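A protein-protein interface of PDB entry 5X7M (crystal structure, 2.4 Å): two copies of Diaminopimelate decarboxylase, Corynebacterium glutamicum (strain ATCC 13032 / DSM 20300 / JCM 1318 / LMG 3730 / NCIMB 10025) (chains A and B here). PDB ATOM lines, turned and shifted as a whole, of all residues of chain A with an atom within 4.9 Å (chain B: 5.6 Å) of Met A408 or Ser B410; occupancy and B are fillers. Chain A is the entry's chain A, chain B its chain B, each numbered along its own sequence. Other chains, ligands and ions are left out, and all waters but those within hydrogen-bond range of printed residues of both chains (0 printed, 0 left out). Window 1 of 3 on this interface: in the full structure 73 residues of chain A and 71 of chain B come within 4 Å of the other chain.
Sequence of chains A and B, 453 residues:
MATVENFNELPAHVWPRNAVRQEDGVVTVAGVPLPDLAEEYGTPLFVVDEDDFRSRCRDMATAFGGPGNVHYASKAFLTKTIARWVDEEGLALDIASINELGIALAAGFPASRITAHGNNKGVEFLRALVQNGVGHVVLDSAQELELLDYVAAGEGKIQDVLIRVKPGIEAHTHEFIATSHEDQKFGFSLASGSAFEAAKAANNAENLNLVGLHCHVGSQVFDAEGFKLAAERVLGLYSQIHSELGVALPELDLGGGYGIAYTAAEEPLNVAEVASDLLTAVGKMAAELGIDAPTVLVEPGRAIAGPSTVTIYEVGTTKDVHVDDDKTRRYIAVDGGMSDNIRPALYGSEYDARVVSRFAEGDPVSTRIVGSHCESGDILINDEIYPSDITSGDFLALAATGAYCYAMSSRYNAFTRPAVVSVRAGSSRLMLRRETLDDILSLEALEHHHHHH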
ATOM      1  N   SER A 339      -3.829  11.831 -17.379  1.00  0.00           N
ATOM      2  CA  SER A 339      -2.861  10.800 -17.709  1.00  0.00           C
ATOM      3  C   SER A 339      -2.537  10.714 -19.196  1.00  0.00           C
ATOM      4  O   SER A 339      -1.454  10.268 -19.495  1.00  0.00           O
ATOM      5  CB  SER A 339      -3.355   9.418 -17.279  1.00  0.00           C
ATOM      6  OG  SER A 339      -4.663   9.209 -17.788  1.00  0.00           O
ATOM      7  N   ILE A 342      -2.062  15.995 -20.042  1.00  0.00           N
ATOM      8  CA  ILE A 342      -1.780  16.747 -18.822  1.00  0.00           C
ATOM      9  C   ILE A 342      -1.857  18.295 -19.034  1.00  0.00           C
ATOM     10  O   ILE A 342      -1.761  19.068 -18.068  1.00  0.00           O
ATOM     11  CB  ILE A 342      -0.357  16.359 -18.346  1.00  0.00           C
ATOM     12  CG1 ILE A 342      -0.036  16.764 -16.890  1.00  0.00           C
ATOM     13  CG2 ILE A 342       0.673  16.983 -19.286  1.00  0.00           C
ATOM     14  CD1 ILE A 342      -0.976  16.203 -15.846  1.00  0.00           C
ATOM     15  N   LEU A 346      -1.590  21.455 -16.564  1.00  0.00           N
ATOM     16  CA  LEU A 346      -0.230  21.933 -16.383  1.00  0.00           C
ATOM     17  C   LEU A 346      -0.088  23.354 -16.912  1.00  0.00           C
ATOM     18  O   LEU A 346       0.395  24.211 -16.214  1.00  0.00           O
ATOM     19  CB  LEU A 346       0.770  20.964 -17.056  1.00  0.00           C
ATOM     20  CG  LEU A 346       2.277  21.275 -16.990  1.00  0.00           C
ATOM     21  CD1 LEU A 346       2.782  21.581 -15.579  1.00  0.00           C
ATOM     22  CD2 LEU A 346       3.057  20.104 -17.585  1.00  0.00           C
ATOM     23  N   TYR A 347      -0.537  23.604 -18.131  1.00  0.00           N
ATOM     24  CA  TYR A 347      -0.321  24.891 -18.797  1.00  0.00           C
ATOM     25  C   TYR A 347      -1.581  25.753 -18.955  1.00  0.00           C
ATOM     26  O   TYR A 347      -1.463  26.891 -19.383  1.00  0.00           O
ATOM     27  CB  TYR A 347       0.282  24.657 -20.192  1.00  0.00           C
ATOM     28  CG  TYR A 347       1.564  23.867 -20.205  1.00  0.00           C
ATOM     29  CD1 TYR A 347       2.752  24.421 -19.701  1.00  0.00           C
ATOM     30  CD2 TYR A 347       1.613  22.574 -20.720  1.00  0.00           C
ATOM     31  CE1 TYR A 347       3.959  23.720 -19.721  1.00  0.00           C
ATOM     32  CE2 TYR A 347       2.822  21.852 -20.728  1.00  0.00           C
ATOM     33  CZ  TYR A 347       3.995  22.439 -20.242  1.00  0.00           C
ATOM     34  OH  TYR A 347       5.198  21.747 -20.235  1.00  0.00           O
ATOM     35  N   TYR A 404       3.150  16.855 -27.635  1.00  0.00           N
ATOM     36  CA  TYR A 404       3.295  16.900 -26.191  1.00  0.00           C
ATOM     37  C   TYR A 404       2.318  16.022 -25.422  1.00  0.00           C
ATOM     38  O   TYR A 404       2.743  15.476 -24.404  1.00  0.00           O
ATOM     39  CB  TYR A 404       3.410  18.355 -25.679  1.00  0.00           C
ATOM     40  CG  TYR A 404       4.573  19.027 -26.374  1.00  0.00           C
ATOM     41  CD1 TYR A 404       5.872  18.585 -26.162  1.00  0.00           C
ATOM     42  CD2 TYR A 404       4.376  19.997 -27.336  1.00  0.00           C
ATOM     43  CE1 TYR A 404       6.942  19.119 -26.847  1.00  0.00           C
ATOM     44  CE2 TYR A 404       5.439  20.557 -28.022  1.00  0.00           C
ATOM     45  CZ  TYR A 404       6.722  20.108 -27.784  1.00  0.00           C
ATOM     46  OH  TYR A 404       7.798  20.657 -28.462  1.00  0.00           O
ATOM     47  N   CYS A 405       1.100  15.756 -25.905  1.00  0.00           N
ATOM     48  CA  CYS A 405       0.199  14.897 -25.161  1.00  0.00           C
ATOM     49  C   CYS A 405       0.676  13.443 -24.874  1.00  0.00           C
ATOM     50  O   CYS A 405       0.964  13.104 -23.741  1.00  0.00           O
ATOM     51  CB  CYS A 405      -1.178  14.941 -25.790  1.00  0.00           C
ATOM     52  SG  CYS A 405      -1.794  16.650 -26.013  1.00  0.00           S
ATOM     53  N   TYR A 406       0.780  12.568 -25.851  1.00  0.00           N
ATOM     54  CA  TYR A 406       1.213  11.215 -25.548  1.00  0.00           C
ATOM     55  C   TYR A 406       2.550  11.151 -24.824  1.00  0.00           C
ATOM     56  O   TYR A 406       2.743  10.304 -23.969  1.00  0.00           O
ATOM     57  CB  TYR A 406       1.313  10.378 -26.816  1.00  0.00           C
ATOM     58  CG  TYR A 406       1.670   8.940 -26.547  1.00  0.00           C
ATOM     59  CD1 TYR A 406       2.993   8.545 -26.504  1.00  0.00           C
ATOM     60  CD2 TYR A 406       0.669   7.959 -26.336  1.00  0.00           C
ATOM     61  CE1 TYR A 406       3.337   7.218 -26.261  1.00  0.00           C
ATOM     62  CE2 TYR A 406       1.007   6.616 -26.072  1.00  0.00           C
ATOM     63  CZ  TYR A 406       2.347   6.271 -26.030  1.00  0.00           C
ATOM     64  OH  TYR A 406       2.757   4.993 -25.831  1.00  0.00           O
ATOM     65  N   ALA A 407       3.473  12.037 -25.166  1.00  0.00           N
ATOM     66  CA  ALA A 407       4.833  12.026 -24.592  1.00  0.00           C
ATOM     67  C   ALA A 407       4.830  12.367 -23.084  1.00  0.00           C
ATOM     68  O   ALA A 407       5.729  11.948 -22.337  1.00  0.00           O
ATOM     69  CB  ALA A 407       5.741  13.000 -25.365  1.00  0.00           C
ATOM     70  N   MET A 408       3.805  13.109 -22.645  1.00  0.00           N
ATOM     71  CA  MET A 408       3.686  13.533 -21.252  1.00  0.00           C
ATOM     72  C   MET A 408       2.676  12.689 -20.492  1.00  0.00           C
ATOM     73  O   MET A 408       2.302  13.042 -19.410  1.00  0.00           O
ATOM     74  CB  MET A 408       3.327  15.046 -21.200  1.00  0.00           C
ATOM     75  CG  MET A 408       4.505  15.880 -21.668  1.00  0.00           C
ATOM     76  SD  MET A 408       4.349  17.655 -21.590  1.00  0.00           S
ATOM     77  CE  MET A 408       4.771  17.853 -19.865  1.00  0.00           C
ATOM     78  N   SER A 409       2.223  11.576 -21.060  1.00  0.00           N
ATOM     79  CA  SER A 409       1.240  10.723 -20.395  1.00  0.00           C
ATOM     80  C   SER A 409       1.875   9.945 -19.245  1.00  0.00           C
ATOM     81  O   SER A 409       3.079   9.654 -19.252  1.00  0.00           O
ATOM     82  CB  SER A 409       0.617   9.732 -21.397  1.00  0.00           C
ATOM     83  OG  SER A 409       1.611   9.021 -22.122  1.00  0.00           O
ATOM     84  N   SER A 410       1.035   9.569 -18.289  1.00  0.00           N
ATOM     85  CA  SER A 410       1.448   8.989 -17.026  1.00  0.00           C
ATOM     86  C   SER A 410       0.527   7.829 -16.736  1.00  0.00           C
ATOM     87  O   SER A 410      -0.472   7.681 -17.408  1.00  0.00           O
ATOM     88  CB  SER A 410       1.271  10.053 -15.942  1.00  0.00           C
ATOM     89  OG  SER A 410      -0.097  10.225 -15.594  1.00  0.00           O
ATOM     90  N   MET B 338      10.964  16.438 -14.201  1.00  0.00           N
ATOM     91  CA  MET B 338       9.517  16.483 -14.142  1.00  0.00           C
ATOM     92  C   MET B 338       8.851  15.176 -14.584  1.00  0.00           C
ATOM     93  O   MET B 338       7.675  14.955 -14.300  1.00  0.00           O
ATOM     94  CB  MET B 338       8.971  17.678 -14.966  1.00  0.00           C
ATOM     95  CG  MET B 338       9.028  17.567 -16.513  1.00  0.00           C
ATOM     96  SD  MET B 338       8.756  19.155 -17.375  1.00  0.00           S
ATOM     97  CE  MET B 338       7.028  19.473 -17.046  1.00  0.00           C
ATOM     98  N   SER B 339       9.595  14.341 -15.306  1.00  0.00           N
ATOM     99  CA  SER B 339       9.202  12.975 -15.600  1.00  0.00           C
ATOM    100  C   SER B 339       9.063  12.165 -14.322  1.00  0.00           C
ATOM    101  O   SER B 339       8.162  11.374 -14.241  1.00  0.00           O
ATOM    102  CB  SER B 339      10.228  12.291 -16.500  1.00  0.00           C
ATOM    103  OG  SER B 339      11.565  12.558 -16.024  1.00  0.00           O
ATOM    104  N   ASP B 340       9.965  12.317 -13.339  1.00  0.00           N
ATOM    105  CA  ASP B 340       9.818  11.548 -12.078  1.00  0.00           C
ATOM    106  C   ASP B 340       9.208  12.356 -10.924  1.00  0.00           C
ATOM    107  O   ASP B 340       8.810  11.768  -9.933  1.00  0.00           O
ATOM    108  CB  ASP B 340      11.109  10.866 -11.657  1.00  0.00           C
ATOM    109  CG  ASP B 340      12.237  11.833 -11.463  1.00  0.00           C
ATOM    110  OD1 ASP B 340      12.353  12.405 -10.345  1.00  0.00           O
ATOM    111  OD2 ASP B 340      13.004  12.009 -12.445  1.00  0.00           O
ATOM    112  N   ILE B 342       6.494  15.625 -11.162  1.00  0.00           N
ATOM    113  CA  ILE B 342       5.781  16.633 -11.935  1.00  0.00           C
ATOM    114  C   ILE B 342       5.198  17.754 -11.043  1.00  0.00           C
ATOM    115  O   ILE B 342       4.714  18.766 -11.555  1.00  0.00           O
ATOM    116  CB  ILE B 342       4.679  15.947 -12.788  1.00  0.00           C
ATOM    117  CG1 ILE B 342       4.124  16.834 -13.922  1.00  0.00           C
ATOM    118  CG2 ILE B 342       3.509  15.517 -11.919  1.00  0.00           C
ATOM    119  CD1 ILE B 342       5.107  17.203 -15.004  1.00  0.00           C
ATOM    120  N   GLU B 375      12.768  21.542 -21.682  1.00  0.00           N
ATOM    121  CA  GLU B 375      11.963  22.721 -21.526  1.00  0.00           C
ATOM    122  C   GLU B 375      12.377  23.448 -20.252  1.00  0.00           C
ATOM    123  O   GLU B 375      12.891  22.838 -19.318  1.00  0.00           O
ATOM    124  CB  GLU B 375      10.466  22.412 -21.524  1.00  0.00           C
ATOM    125  CG  GLU B 375      10.006  21.259 -20.663  1.00  0.00           C
ATOM    126  CD  GLU B 375       8.476  21.104 -20.706  1.00  0.00           C
ATOM    127  OE1 GLU B 375       7.989  20.070 -21.239  1.00  0.00           O
ATOM    128  OE2 GLU B 375       7.754  22.024 -20.220  1.00  0.00           O
ATOM    129  N   MET B 408       2.604   9.750 -10.876  1.00  0.00           N
ATOM    130  CA  MET B 408       2.407  10.746 -11.937  1.00  0.00           C
ATOM    131  C   MET B 408       3.579  10.818 -12.949  1.00  0.00           C
ATOM    132  O   MET B 408       3.577  11.673 -13.813  1.00  0.00           O
ATOM    133  CB  MET B 408       2.152  12.117 -11.280  1.00  0.00           C
ATOM    134  CG  MET B 408       0.936  12.065 -10.385  1.00  0.00           C
ATOM    135  SD  MET B 408       0.265  13.638  -9.924  1.00  0.00           S
ATOM    136  CE  MET B 408      -1.018  13.775 -11.154  1.00  0.00           C
ATOM    137  N   SER B 409       4.551   9.909 -12.855  1.00  0.00           N
ATOM    138  CA  SER B 409       5.692   9.914 -13.724  1.00  0.00           C
ATOM    139  C   SER B 409       5.350   9.631 -15.211  1.00  0.00           C
ATOM    140  O   SER B 409       4.435   8.850 -15.525  1.00  0.00           O
ATOM    141  CB  SER B 409       6.772   8.922 -13.221  1.00  0.00           C
ATOM    142  OG  SER B 409       6.325   7.569 -13.215  1.00  0.00           O
ATOM    143  N   SER B 410       6.120  10.274 -16.097  1.00  0.00           N
ATOM    144  CA  SER B 410       5.919  10.250 -17.536  1.00  0.00           C
ATOM    145  C   SER B 410       7.163   9.774 -18.243  1.00  0.00           C
ATOM    146  O   SER B 410       8.220   9.632 -17.638  1.00  0.00           O
ATOM    147  CB  SER B 410       5.646  11.675 -18.001  1.00  0.00           C
ATOM    148  OG  SER B 410       6.854  12.410 -18.129  1.00  0.00           O
ATOM    149  N   ARG B 411       7.042   9.590 -19.545  1.00  0.00           N
ATOM    150  CA  ARG B 411       8.168   9.199 -20.403  1.00  0.00           C
ATOM    151  C   ARG B 411       8.623  10.341 -21.298  1.00  0.00           C
ATOM    152  O   ARG B 411       9.255  10.106 -22.322  1.00  0.00           O
ATOM    153  CB  ARG B 411       7.793   7.983 -21.258  1.00  0.00           C
ATOM    154  CG  ARG B 411       7.618   6.715 -20.460  1.00  0.00           C
ATOM    155  CD  ARG B 411       7.182   5.596 -21.381  1.00  0.00           C
ATOM    156  NE  ARG B 411       7.353   4.309 -20.722  1.00  0.00           N
ATOM    157  CZ  ARG B 411       6.861   3.149 -21.163  1.00  0.00           C
ATOM    158  NH1 ARG B 411       6.156   3.085 -22.300  1.00  0.00           N
ATOM    159  NH2 ARG B 411       7.067   2.035 -20.461  1.00  0.00           N
ATOM    160  N   TYR B 412       8.339  11.573 -20.880  1.00  0.00           N
ATOM    161  CA  TYR B 412       8.757  12.764 -21.613  1.00  0.00           C
ATOM    162  C   TYR B 412      10.240  12.681 -21.961  1.00  0.00           C
ATOM    163  O   TYR B 412      11.070  12.260 -21.137  1.00  0.00           O
ATOM    164  CB  TYR B 412       8.436  14.059 -20.816  1.00  0.00           C
ATOM    165  CG  TYR B 412       8.578  15.308 -21.650  1.00  0.00           C
ATOM    166  CD1 TYR B 412       7.923  15.415 -22.867  1.00  0.00           C
ATOM    167  CD2 TYR B 412       9.381  16.370 -21.246  1.00  0.00           C
ATOM    168  CE1 TYR B 412       8.045  16.525 -23.664  1.00  0.00           C
ATOM    169  CE2 TYR B 412       9.517  17.510 -22.049  1.00  0.00           C
ATOM    170  CZ  TYR B 412       8.840  17.577 -23.271  1.00  0.00           C
ATOM    171  OH  TYR B 412       8.930  18.669 -24.139  1.00  0.00           O
ATOM    172  N   PHE B 415      12.457   9.427 -21.275  1.00  0.00           N
ATOM    173  CA  PHE B 415      13.070   8.997 -20.003  1.00  0.00           C
ATOM    174  C   PHE B 415      12.352   7.767 -19.411  1.00  0.00           C
ATOM    175  O   PHE B 415      11.141   7.572 -19.546  1.00  0.00           O
ATOM    176  CB  PHE B 415      13.012  10.096 -18.940  1.00  0.00           C
ATOM    177  CG  PHE B 415      14.043  11.183 -19.087  1.00  0.00           C
ATOM    178  CD1 PHE B 415      14.500  11.618 -20.342  1.00  0.00           C
ATOM    179  CD2 PHE B 415      14.486  11.859 -17.950  1.00  0.00           C
ATOM    180  CE1 PHE B 415      15.406  12.668 -20.436  1.00  0.00           C
ATOM    181  CE2 PHE B 415      15.395  12.904 -18.037  1.00  0.00           C
ATOM    182  CZ  PHE B 415      15.858  13.316 -19.276  1.00  0.00           C
ATOM    183  N   THR B 416      13.120   6.942 -18.727  1.00  0.00           N
ATOM    184  CA  THR B 416      12.600   5.708 -18.224  1.00  0.00           C
ATOM    185  C   THR B 416      12.152   5.976 -16.827  1.00  0.00           C
ATOM    186  O   THR B 416      12.795   6.691 -16.104  1.00  0.00           O
ATOM    187  CB  THR B 416      13.656   4.575 -18.314  1.00  0.00           C
ATOM    188  OG1 THR B 416      14.956   5.053 -17.933  1.00  0.00           O
ATOM    189  CG2 THR B 416      13.732   4.063 -19.753  1.00  0.00           C
ATOM    190  N   ARG B 417      11.005   5.454 -16.464  1.00  0.00           N
ATOM    191  CA  ARG B 417      10.543   5.504 -15.075  1.00  0.00           C
ATOM    192  C   ARG B 417      11.646   4.935 -14.130  1.00  0.00           C
ATOM    193  O   ARG B 417      12.224   3.866 -14.405  1.00  0.00           O
ATOM    194  CB  ARG B 417       9.254   4.688 -14.971  1.00  0.00           C
ATOM    195  CG  ARG B 417       8.304   5.008 -13.840  1.00  0.00           C
ATOM    196  CD  ARG B 417       6.910   4.394 -14.083  1.00  0.00           C
ATOM    197  NE  ARG B 417       6.640   4.310 -15.517  1.00  0.00           N
ATOM    198  CZ  ARG B 417       6.052   5.236 -16.287  1.00  0.00           C
ATOM    199  NH1 ARG B 417       5.560   6.374 -15.798  1.00  0.00           N
ATOM    200  NH2 ARG B 417       5.951   4.999 -17.585  1.00  0.00           N
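The backbone carbonyl oxygen (O) of Ala A407 lies within hydrogen-bond range of the backbone NH (N) of Tyr B412 (3.0 Å).
The side-chain hydroxyl (OH) of Tyr A347 lies within hydrogen-bond range of the side-chain carboxylate (OE2) of Glu B375 (2.6 Å).
The backbone carbonyl oxygen of Ser B409 lies within hydrogen-bond range of the guanidinium group of Arg B417 (2.7 Å).
The backbone carbonyl oxygen (O) of Ser B339 lies within hydrogen-bond range of the backbone NH (N) of Ser B410 (3.0 Å).
The side-chain hydroxyl (OG) of Ser B410 lies within hydrogen-bond range of the backbone NH (N) of Tyr B412, at 3.2 Å.
The backbone carbonyl oxygen (O) of Ser A339 is in hydrogen-bond range of the backbone NH (N) of Ser A410, at 2.9 Å.
The side-chain carboxylate (OE1) of Glu B375 sits close to the side-chain hydroxyl (OH) of Tyr B412, 3.4 Å away.
The backbone carbonyl oxygen (O) of Tyr A406 sits at hydrogen-bond distance from the side-chain hydroxyl (OG) of Ser A409 (2.5 Å).
Among the printed residues, merely in contact across the chains: Tyr A404 with Tyr B412 (3.4 Å), Ala A407 with Arg B411 (3.5 Å), Met A408 with Met B338 (3.96 Å), Met A408 with Ser B410 (3.9 Å), Met A408 with Tyr B412 (3.7 Å), Ser A409 with Ser B410 (3.4 Å), Ser A409 with Arg B411 (3.97 Å), Ser A410 with Met B408 (3.5 Å) and Ser A410 with Ser B409 (3.3 Å).
Printed residues of chain B within 4 Å of Tyr A347: Glu B375.
Printed residues of chain B within 4 Å of Ala A407: Arg B411 and Tyr B412.
Met A408 touches just these residues of chain B: Met B338, Ser B410 and Tyr B412.
Of the printed residues of chain B, Ser A410 touches Met B408 (3.5 Å) and Ser B409 (3.3 Å).
Asp B340 touches none of the printed residues of chain A.
The nearest residue of chain A that does not touch Ser B410 is Ala A407 (4.3 Å).
The nearest printed residue of chain A that does not touch Glu B375 is Met A408 (4.1 Å).
Of the 11 printed residues of chain A, 6 touch a printed residue of chain B.
Hydrophobic or aromatic side chains of chain A within 4 Å of the printed part of chain B: Tyr A347, Tyr A404 and Met A408.
Of the 13 printed residues of chain B, 7 touch a printed residue of chain A.
Hydrophobic or aromatic side chains of chain B that line the printed part of chain A: Met B338 and Tyr B412.
Met A408 touches Ser B410, and with the chains exchanged Ser A410 touches Met B408.
Ser A409 touches Ser B410, and with the chains exchanged Ser A410 touches Ser B409.
5 positions are printed for both chains.
Of the 11 pairs that touch across the chains among the printed residues, 4 have their exchanged pair printed and touching as well.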
